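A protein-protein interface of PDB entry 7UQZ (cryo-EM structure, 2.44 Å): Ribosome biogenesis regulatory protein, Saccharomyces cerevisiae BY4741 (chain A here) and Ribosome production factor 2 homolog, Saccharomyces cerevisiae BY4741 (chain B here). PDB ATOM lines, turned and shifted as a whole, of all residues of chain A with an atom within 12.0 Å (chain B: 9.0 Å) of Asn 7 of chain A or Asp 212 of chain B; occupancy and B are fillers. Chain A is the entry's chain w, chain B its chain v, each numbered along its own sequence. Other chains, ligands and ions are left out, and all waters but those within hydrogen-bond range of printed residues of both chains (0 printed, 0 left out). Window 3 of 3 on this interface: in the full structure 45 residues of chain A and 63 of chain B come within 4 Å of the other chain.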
ATOM      1  N   ASN A   7       2.472  29.897 -25.252  1.00  0.00           N
ATOM      2  CA  ASN A   7       3.065  28.977 -24.289  1.00  0.00           C
ATOM      3  C   ASN A   7       4.329  28.327 -24.850  1.00  0.00           C
ATOM      4  O   ASN A   7       4.368  27.121 -25.100  1.00  0.00           O
ATOM      5  CB  ASN A   7       2.048  27.907 -23.880  1.00  0.00           C
ATOM      6  CG  ASN A   7       1.352  27.273 -25.069  1.00  0.00           C
ATOM      7  OD1 ASN A   7       0.260  27.688 -25.457  1.00  0.00           O
ATOM      8  ND2 ASN A   7       1.983  26.261 -25.652  1.00  0.00           N
ATOM      9  N   LEU A   8       5.363  29.139 -25.043  1.00  0.00           N
ATOM     10  CA  LEU A   8       6.605  28.637 -25.609  1.00  0.00           C
ATOM     11  C   LEU A   8       7.313  27.724 -24.611  1.00  0.00           C
ATOM     12  O   LEU A   8       7.258  27.964 -23.401  1.00  0.00           O
ATOM     13  CB  LEU A   8       7.513  29.798 -26.007  1.00  0.00           C
ATOM     14  CG  LEU A   8       6.875  30.782 -26.989  1.00  0.00           C
ATOM     15  CD1 LEU A   8       7.858  31.866 -27.402  1.00  0.00           C
ATOM     16  CD2 LEU A   8       6.337  30.050 -28.206  1.00  0.00           C
ATOM     17  N   PRO A   9       7.967  26.666 -25.082  1.00  0.00           N
ATOM     18  CA  PRO A   9       8.597  25.714 -24.161  1.00  0.00           C
ATOM     19  C   PRO A   9       9.845  26.286 -23.504  1.00  0.00           C
ATOM     20  O   PRO A   9      10.422  27.283 -23.944  1.00  0.00           O
ATOM     21  CB  PRO A   9       8.946  24.522 -25.061  1.00  0.00           C
ATOM     22  CG  PRO A   9       8.104  24.699 -26.295  1.00  0.00           C
ATOM     23  CD  PRO A   9       7.974  26.177 -26.469  1.00  0.00           C
ATOM     24  N   VAL A  10      10.255  25.627 -22.423  1.00  0.00           N
ATOM     25  CA  VAL A  10      11.474  25.967 -21.705  1.00  0.00           C
ATOM     26  C   VAL A  10      12.505  24.844 -21.804  1.00  0.00           C
ATOM     27  O   VAL A  10      13.455  24.804 -21.025  1.00  0.00           O
ATOM     28  CB  VAL A  10      11.178  26.320 -20.239  1.00  0.00           C
ATOM     29  CG1 VAL A  10      10.328  27.575 -20.155  1.00  0.00           C
ATOM     30  CG2 VAL A  10      10.490  25.156 -19.543  1.00  0.00           C
ATOM     31  N   THR A  11      12.330  23.931 -22.753  1.00  0.00           N
ATOM     32  CA  THR A  11      13.214  22.781 -22.935  1.00  0.00           C
ATOM     33  C   THR A  11      14.066  23.026 -24.174  1.00  0.00           C
ATOM     34  O   THR A  11      13.575  22.939 -25.303  1.00  0.00           O
ATOM     35  CB  THR A  11      12.410  21.490 -23.063  1.00  0.00           C
ATOM     36  OG1 THR A  11      11.593  21.551 -24.240  1.00  0.00           O
ATOM     37  CG2 THR A  11      11.517  21.299 -21.850  1.00  0.00           C
ATOM     38  N   VAL A  12      15.342  23.332 -23.962  1.00  0.00           N
ATOM     39  CA  VAL A  12      16.270  23.600 -25.054  1.00  0.00           C
ATOM     40  C   VAL A  12      17.069  22.335 -25.340  1.00  0.00           C
ATOM     41  O   VAL A  12      17.712  21.778 -24.443  1.00  0.00           O
ATOM     42  CB  VAL A  12      17.200  24.774 -24.716  1.00  0.00           C
ATOM     43  CG1 VAL A  12      18.146  25.047 -25.870  1.00  0.00           C
ATOM     44  CG2 VAL A  12      16.385  26.013 -24.388  1.00  0.00           C
ATOM     45  N   ARG A  54      19.576  33.581 -25.867  1.00  0.00           N
ATOM     46  CA  ARG A  54      18.313  33.264 -25.215  1.00  0.00           C
ATOM     47  C   ARG A  54      18.293  31.815 -24.752  1.00  0.00           C
ATOM     48  O   ARG A  54      17.882  31.519 -23.626  1.00  0.00           O
ATOM     49  CB  ARG A  54      17.157  33.548 -26.177  1.00  0.00           C
ATOM     50  CG  ARG A  54      15.851  33.992 -25.535  1.00  0.00           C
ATOM     51  CD  ARG A  54      15.092  32.830 -24.928  1.00  0.00           C
ATOM     52  NE  ARG A  54      14.912  31.737 -25.874  1.00  0.00           N
ATOM     53  CZ  ARG A  54      14.320  30.587 -25.583  1.00  0.00           C
ATOM     54  NH1 ARG A  54      13.820  30.353 -24.380  1.00  0.00           N
ATOM     55  NH2 ARG A  54      14.228  29.648 -26.519  1.00  0.00           N
ATOM     56  N   GLN A  58      18.279  30.693 -20.893  1.00  0.00           N
ATOM     57  CA  GLN A  58      17.191  29.835 -20.436  1.00  0.00           C
ATOM     58  C   GLN A  58      17.725  28.616 -19.692  1.00  0.00           C
ATOM     59  O   GLN A  58      17.215  28.261 -18.622  1.00  0.00           O
ATOM     60  CB  GLN A  58      16.330  29.405 -21.624  1.00  0.00           C
ATOM     61  CG  GLN A  58      15.229  28.413 -21.283  1.00  0.00           C
ATOM     62  CD  GLN A  58      14.043  29.062 -20.599  1.00  0.00           C
ATOM     63  OE1 GLN A  58      13.310  29.840 -21.208  1.00  0.00           O
ATOM     64  NE2 GLN A  58      13.847  28.744 -19.326  1.00  0.00           N
ATOM     65  N   ASN A  62      17.263  27.785 -15.741  1.00  0.00           N
ATOM     66  CA  ASN A  62      16.737  26.492 -15.313  1.00  0.00           C
ATOM     67  C   ASN A  62      17.618  25.864 -14.239  1.00  0.00           C
ATOM     68  O   ASN A  62      17.113  25.362 -13.227  1.00  0.00           O
ATOM     69  CB  ASN A  62      16.604  25.554 -16.512  1.00  0.00           C
ATOM     70  CG  ASN A  62      15.470  25.947 -17.438  1.00  0.00           C
ATOM     71  OD1 ASN A  62      14.863  27.006 -17.284  1.00  0.00           O
ATOM     72  ND2 ASN A  62      15.182  25.093 -18.413  1.00  0.00           N
ATOM     73  N   TYR B 209       7.977  35.118 -18.447  1.00  0.00           N
ATOM     74  CA  TYR B 209       6.553  34.943 -18.685  1.00  0.00           C
ATOM     75  C   TYR B 209       6.160  33.525 -18.302  1.00  0.00           C
ATOM     76  O   TYR B 209       7.001  32.625 -18.238  1.00  0.00           O
ATOM     77  CB  TYR B 209       6.174  35.205 -20.150  1.00  0.00           C
ATOM     78  CG  TYR B 209       6.626  36.542 -20.692  1.00  0.00           C
ATOM     79  CD1 TYR B 209       5.823  37.669 -20.576  1.00  0.00           C
ATOM     80  CD2 TYR B 209       7.853  36.675 -21.329  1.00  0.00           C
ATOM     81  CE1 TYR B 209       6.232  38.894 -21.073  1.00  0.00           C
ATOM     82  CE2 TYR B 209       8.269  37.893 -21.829  1.00  0.00           C
ATOM     83  CZ  TYR B 209       7.456  38.997 -21.700  1.00  0.00           C
ATOM     84  OH  TYR B 209       7.872  40.211 -22.198  1.00  0.00           O
ATOM     85  N   LYS B 210       4.869  33.336 -18.041  1.00  0.00           N
ATOM     86  CA  LYS B 210       4.349  32.002 -17.776  1.00  0.00           C
ATOM     87  C   LYS B 210       4.483  31.135 -19.022  1.00  0.00           C
ATOM     88  O   LYS B 210       4.183  31.571 -20.137  1.00  0.00           O
ATOM     89  CB  LYS B 210       2.888  32.076 -17.340  1.00  0.00           C
ATOM     90  CG  LYS B 210       2.400  30.854 -16.580  1.00  0.00           C
ATOM     91  CD  LYS B 210       3.135  30.706 -15.260  1.00  0.00           C
ATOM     92  CE  LYS B 210       2.567  29.567 -14.433  1.00  0.00           C
ATOM     93  NZ  LYS B 210       1.129  29.779 -14.108  1.00  0.00           N
ATOM     94  N   SER B 211       4.942  29.901 -18.829  1.00  0.00           N
ATOM     95  CA  SER B 211       5.217  29.008 -19.948  1.00  0.00           C
ATOM     96  C   SER B 211       4.103  28.010 -20.217  1.00  0.00           C
ATOM     97  O   SER B 211       4.018  27.493 -21.337  1.00  0.00           O
ATOM     98  CB  SER B 211       6.520  28.238 -19.706  1.00  0.00           C
ATOM     99  OG  SER B 211       6.367  27.291 -18.662  1.00  0.00           O
ATOM    100  N   ASP B 212       3.289  27.691 -19.205  1.00  0.00           N
ATOM    101  CA  ASP B 212       2.158  26.768 -19.306  1.00  0.00           C
ATOM    102  C   ASP B 212       2.606  25.349 -19.658  1.00  0.00           C
ATOM    103  O   ASP B 212       1.773  24.477 -19.924  1.00  0.00           O
ATOM    104  CB  ASP B 212       1.132  27.287 -20.324  1.00  0.00           C
ATOM    105  CG  ASP B 212      -0.260  26.732 -20.091  1.00  0.00           C
ATOM    106  OD1 ASP B 212      -0.467  26.028 -19.081  1.00  0.00           O
ATOM    107  OD2 ASP B 212      -1.152  27.006 -20.922  1.00  0.00           O
ATOM    108  N   GLN B 213       3.917  25.103 -19.660  1.00  0.00           N
ATOM    109  CA  GLN B 213       4.466  23.775 -19.900  1.00  0.00           C
ATOM    110  C   GLN B 213       5.569  23.378 -18.934  1.00  0.00           C
ATOM    111  O   GLN B 213       5.785  22.176 -18.741  1.00  0.00           O
ATOM    112  CB  GLN B 213       5.008  23.663 -21.333  1.00  0.00           C
ATOM    113  CG  GLN B 213       3.937  23.708 -22.412  1.00  0.00           C
ATOM    114  CD  GLN B 213       4.503  23.519 -23.805  1.00  0.00           C
ATOM    115  OE1 GLN B 213       5.719  23.446 -23.988  1.00  0.00           O
ATOM    116  NE2 GLN B 213       3.623  23.436 -24.795  1.00  0.00           N
ATOM    117  N   GLY B 214       6.270  24.331 -18.325  1.00  0.00           N
ATOM    118  CA  GLY B 214       7.278  24.017 -17.333  1.00  0.00           C
ATOM    119  C   GLY B 214       6.770  24.246 -15.927  1.00  0.00           C
ATOM    120  O   GLY B 214       7.555  24.311 -14.975  1.00  0.00           O
ATOM    121  N   GLY B 215       5.453  24.374 -15.787  1.00  0.00           N
ATOM    122  CA  GLY B 215       4.847  24.632 -14.500  1.00  0.00           C
ATOM    123  C   GLY B 215       5.017  26.079 -14.063  1.00  0.00           C
ATOM    124  O   GLY B 215       5.409  26.960 -14.828  1.00  0.00           O
ATOM    125  N   LYS B 216       4.710  26.308 -12.788  1.00  0.00           N
ATOM    126  CA  LYS B 216       4.835  27.626 -12.182  1.00  0.00           C
ATOM    127  C   LYS B 216       6.212  27.858 -11.574  1.00  0.00           C
ATOM    128  O   LYS B 216       6.431  28.894 -10.941  1.00  0.00           O
ATOM    129  CB  LYS B 216       3.753  27.824 -11.116  1.00  0.00           C
ATOM    130  CG  LYS B 216       3.848  26.866  -9.944  1.00  0.00           C
ATOM    131  CD  LYS B 216       2.719  27.092  -8.949  1.00  0.00           C
ATOM    132  CE  LYS B 216       2.782  28.486  -8.342  1.00  0.00           C
ATOM    133  NZ  LYS B 216       4.085  28.738  -7.667  1.00  0.00           N
ATOM    134  N   ARG B 217       7.139  26.915 -11.752  1.00  0.00           N
ATOM    135  CA  ARG B 217       8.497  27.053 -11.251  1.00  0.00           C
ATOM    136  C   ARG B 217       9.518  27.357 -12.336  1.00  0.00           C
ATOM    137  O   ARG B 217      10.627  27.789 -12.010  1.00  0.00           O
ATOM    138  CB  ARG B 217       8.922  25.771 -10.520  1.00  0.00           C
ATOM    139  CG  ARG B 217       7.845  25.194  -9.619  1.00  0.00           C
ATOM    140  CD  ARG B 217       7.622  26.060  -8.395  1.00  0.00           C
ATOM    141  NE  ARG B 217       8.732  25.960  -7.456  1.00  0.00           N
ATOM    142  CZ  ARG B 217       8.795  25.083  -6.466  1.00  0.00           C
ATOM    143  NH1 ARG B 217       7.819  24.217  -6.246  1.00  0.00           N
ATOM    144  NH2 ARG B 217       9.864  25.073  -5.675  1.00  0.00           N
ATOM    145  N   LEU B 218       9.180  27.142 -13.606  1.00  0.00           N
ATOM    146  CA  LEU B 218      10.095  27.377 -14.723  1.00  0.00           C
ATOM    147  C   LEU B 218       9.448  28.313 -15.734  1.00  0.00           C
ATOM    148  O   LEU B 218       8.652  27.864 -16.578  1.00  0.00           O
ATOM    149  CB  LEU B 218      10.484  26.059 -15.389  1.00  0.00           C
ATOM    150  CG  LEU B 218      11.150  25.024 -14.482  1.00  0.00           C
ATOM    151  CD1 LEU B 218      11.454  23.755 -15.257  1.00  0.00           C
ATOM    152  CD2 LEU B 218      12.415  25.594 -13.860  1.00  0.00           C
ATOM    153  N   PRO B 219       9.743  29.608 -15.692  1.00  0.00           N
ATOM    154  CA  PRO B 219       9.148  30.545 -16.648  1.00  0.00           C
ATOM    155  C   PRO B 219       9.942  30.645 -17.944  1.00  0.00           C
ATOM    156  O   PRO B 219      11.144  30.378 -18.000  1.00  0.00           O
ATOM    157  CB  PRO B 219       9.188  31.876 -15.886  1.00  0.00           C
ATOM    158  CG  PRO B 219      10.404  31.758 -15.037  1.00  0.00           C
ATOM    159  CD  PRO B 219      10.528  30.302 -14.655  1.00  0.00           C
ATOM    160  N   ARG B 220       9.231  31.041 -18.999  1.00  0.00           N
ATOM    161  CA  ARG B 220       9.860  31.272 -20.293  1.00  0.00           C
ATOM    162  C   ARG B 220      10.678  32.556 -20.256  1.00  0.00           C
ATOM    163  O   ARG B 220      10.193  33.600 -19.812  1.00  0.00           O
ATOM    164  CB  ARG B 220       8.795  31.347 -21.388  1.00  0.00           C
ATOM    165  CG  ARG B 220       9.295  31.862 -22.732  1.00  0.00           C
ATOM    166  CD  ARG B 220      10.061  30.800 -23.505  1.00  0.00           C
ATOM    167  NE  ARG B 220      10.481  31.294 -24.811  1.00  0.00           N
ATOM    168  CZ  ARG B 220      11.054  30.553 -25.750  1.00  0.00           C
ATOM    169  NH1 ARG B 220      11.286  29.263 -25.566  1.00  0.00           N
ATOM    170  NH2 ARG B 220      11.402  31.120 -26.901  1.00  0.00           N
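O of Val 10 of chain A is in hydrogen-bond range of ND2 of Asn 62 of chain A (3.1 Å). O of Leu 218 of chain B is in hydrogen-bond range of OG of Ser 211 of chain B, at 3.1 Å. The side-chain hydroxyl of Ser 211 of chain B sits close to the backbone NH of Gln 213 of chain B (3.4 Å). The side-chain amide oxygen (OD1) of Asn 62 of chain A is in hydrogen-bond range of the side-chain amide nitrogen (NE2) of Gln 58 of chain A (2.9 Å). The side-chain hydroxyl (OG) of Ser 211 of chain B sits at hydrogen-bond distance from the backbone NH (N) of Gly 214 of chain B (3.0 Å). The backbone carbonyl oxygen (O) of Tyr 209 of chain B lies within hydrogen-bond range of the backbone NH (N) of Arg 220 of chain B, at 2.8 Å.
NE2 of Gln 58 of chain A is in hydrogen-bond range of O of Pro 219 of chain B (3.4 Å). The guanidinium group (NH1) of Arg 54 of chain A lies close to the guanidinium group (NH1) of Arg 220 of chain B (3.0 Å). NH1 of Arg 220 of chain B is in hydrogen-bond range of O of Pro 9 of chain A, 2.7 Å away. The side-chain amide nitrogen (NE2) of Gln 213 of chain B lies close to the side-chain amide nitrogen (ND2) of Asn 7 of chain A (3.4 Å).
CB of Asn 7 of chain A touches O of Ser 211 of chain B, at 3.2 Å. CB of Asp 212 of chain B touches CB of Asn 7 of chain A, at 3.7 Å. Ser 211 of chain B touches Leu 8 of chain A (CB to O, 3.8 Å). Arg 220 of chain B touches Leu 8 of chain A. Pro 9 of chain A touches Gln 213 of chain B (CG to OE1, 3.5 Å). Val 10 of chain A touches Ser 211 of chain B (CG1 to CB, 3.9 Å). Val 10 of chain A touches Leu 218 of chain B. Pro 219 of chain B touches Val 10 of chain A (O to CG1, 3.6 Å). CG1 of Val 10 of chain A touches CA of Arg 220 of chain B, at 3.7 Å. Gln 58 of chain A touches Arg 220 of chain B (OE1 to CA, 3.8 Å).
Printed residues of chain A that touch a printed residue of chain B: Asn 7, Leu 8, Pro 9, Val 10, Arg 54 and Gln 58. Along chain A the printed residues that touch a printed residue of chain B span positions 7 to 58. Among the printed residues, 14 pairs touch across the chains.
Asn 7 of chain A touches three residues of chain B. Of chain A, only Asn 7 (3.7 Å) comes within 4 Å of Asp 212 of chain B. Of chain A, only Asn 7 (3.4 Å) and Pro 9 (3.5 Å) come within 4 Å of Gln 213 of chain B. No residue of chain A comes within 4 Å of Gly 214 of chain B. No residue of chain A comes within 4 Å of Gly 215 of chain B. Of the printed residues of chain B, Arg 54 of chain A touches Arg 220 (3.0 Å). Of the printed residues of chain A, Arg 220 of chain B touches Leu 8 (3.5 Å), Pro 9 (2.7 Å), Val 10 (3.7 Å), Arg 54 (3.0 Å) and Gln 58 (3.8 Å). Printed residues of chain B within 4 Å of Leu 8 of chain A: Ser 211 (3.8 Å) and Arg 220 (3.5 Å). Printed residues of chain A within 4 Å of Pro 219 of chain B: Val 10 (3.6 Å) and Gln 58 (3.4 Å). Of the printed residues of chain B, Pro 9 of chain A touches Gln 213 (3.5 Å) and Arg 220 (2.7 Å).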
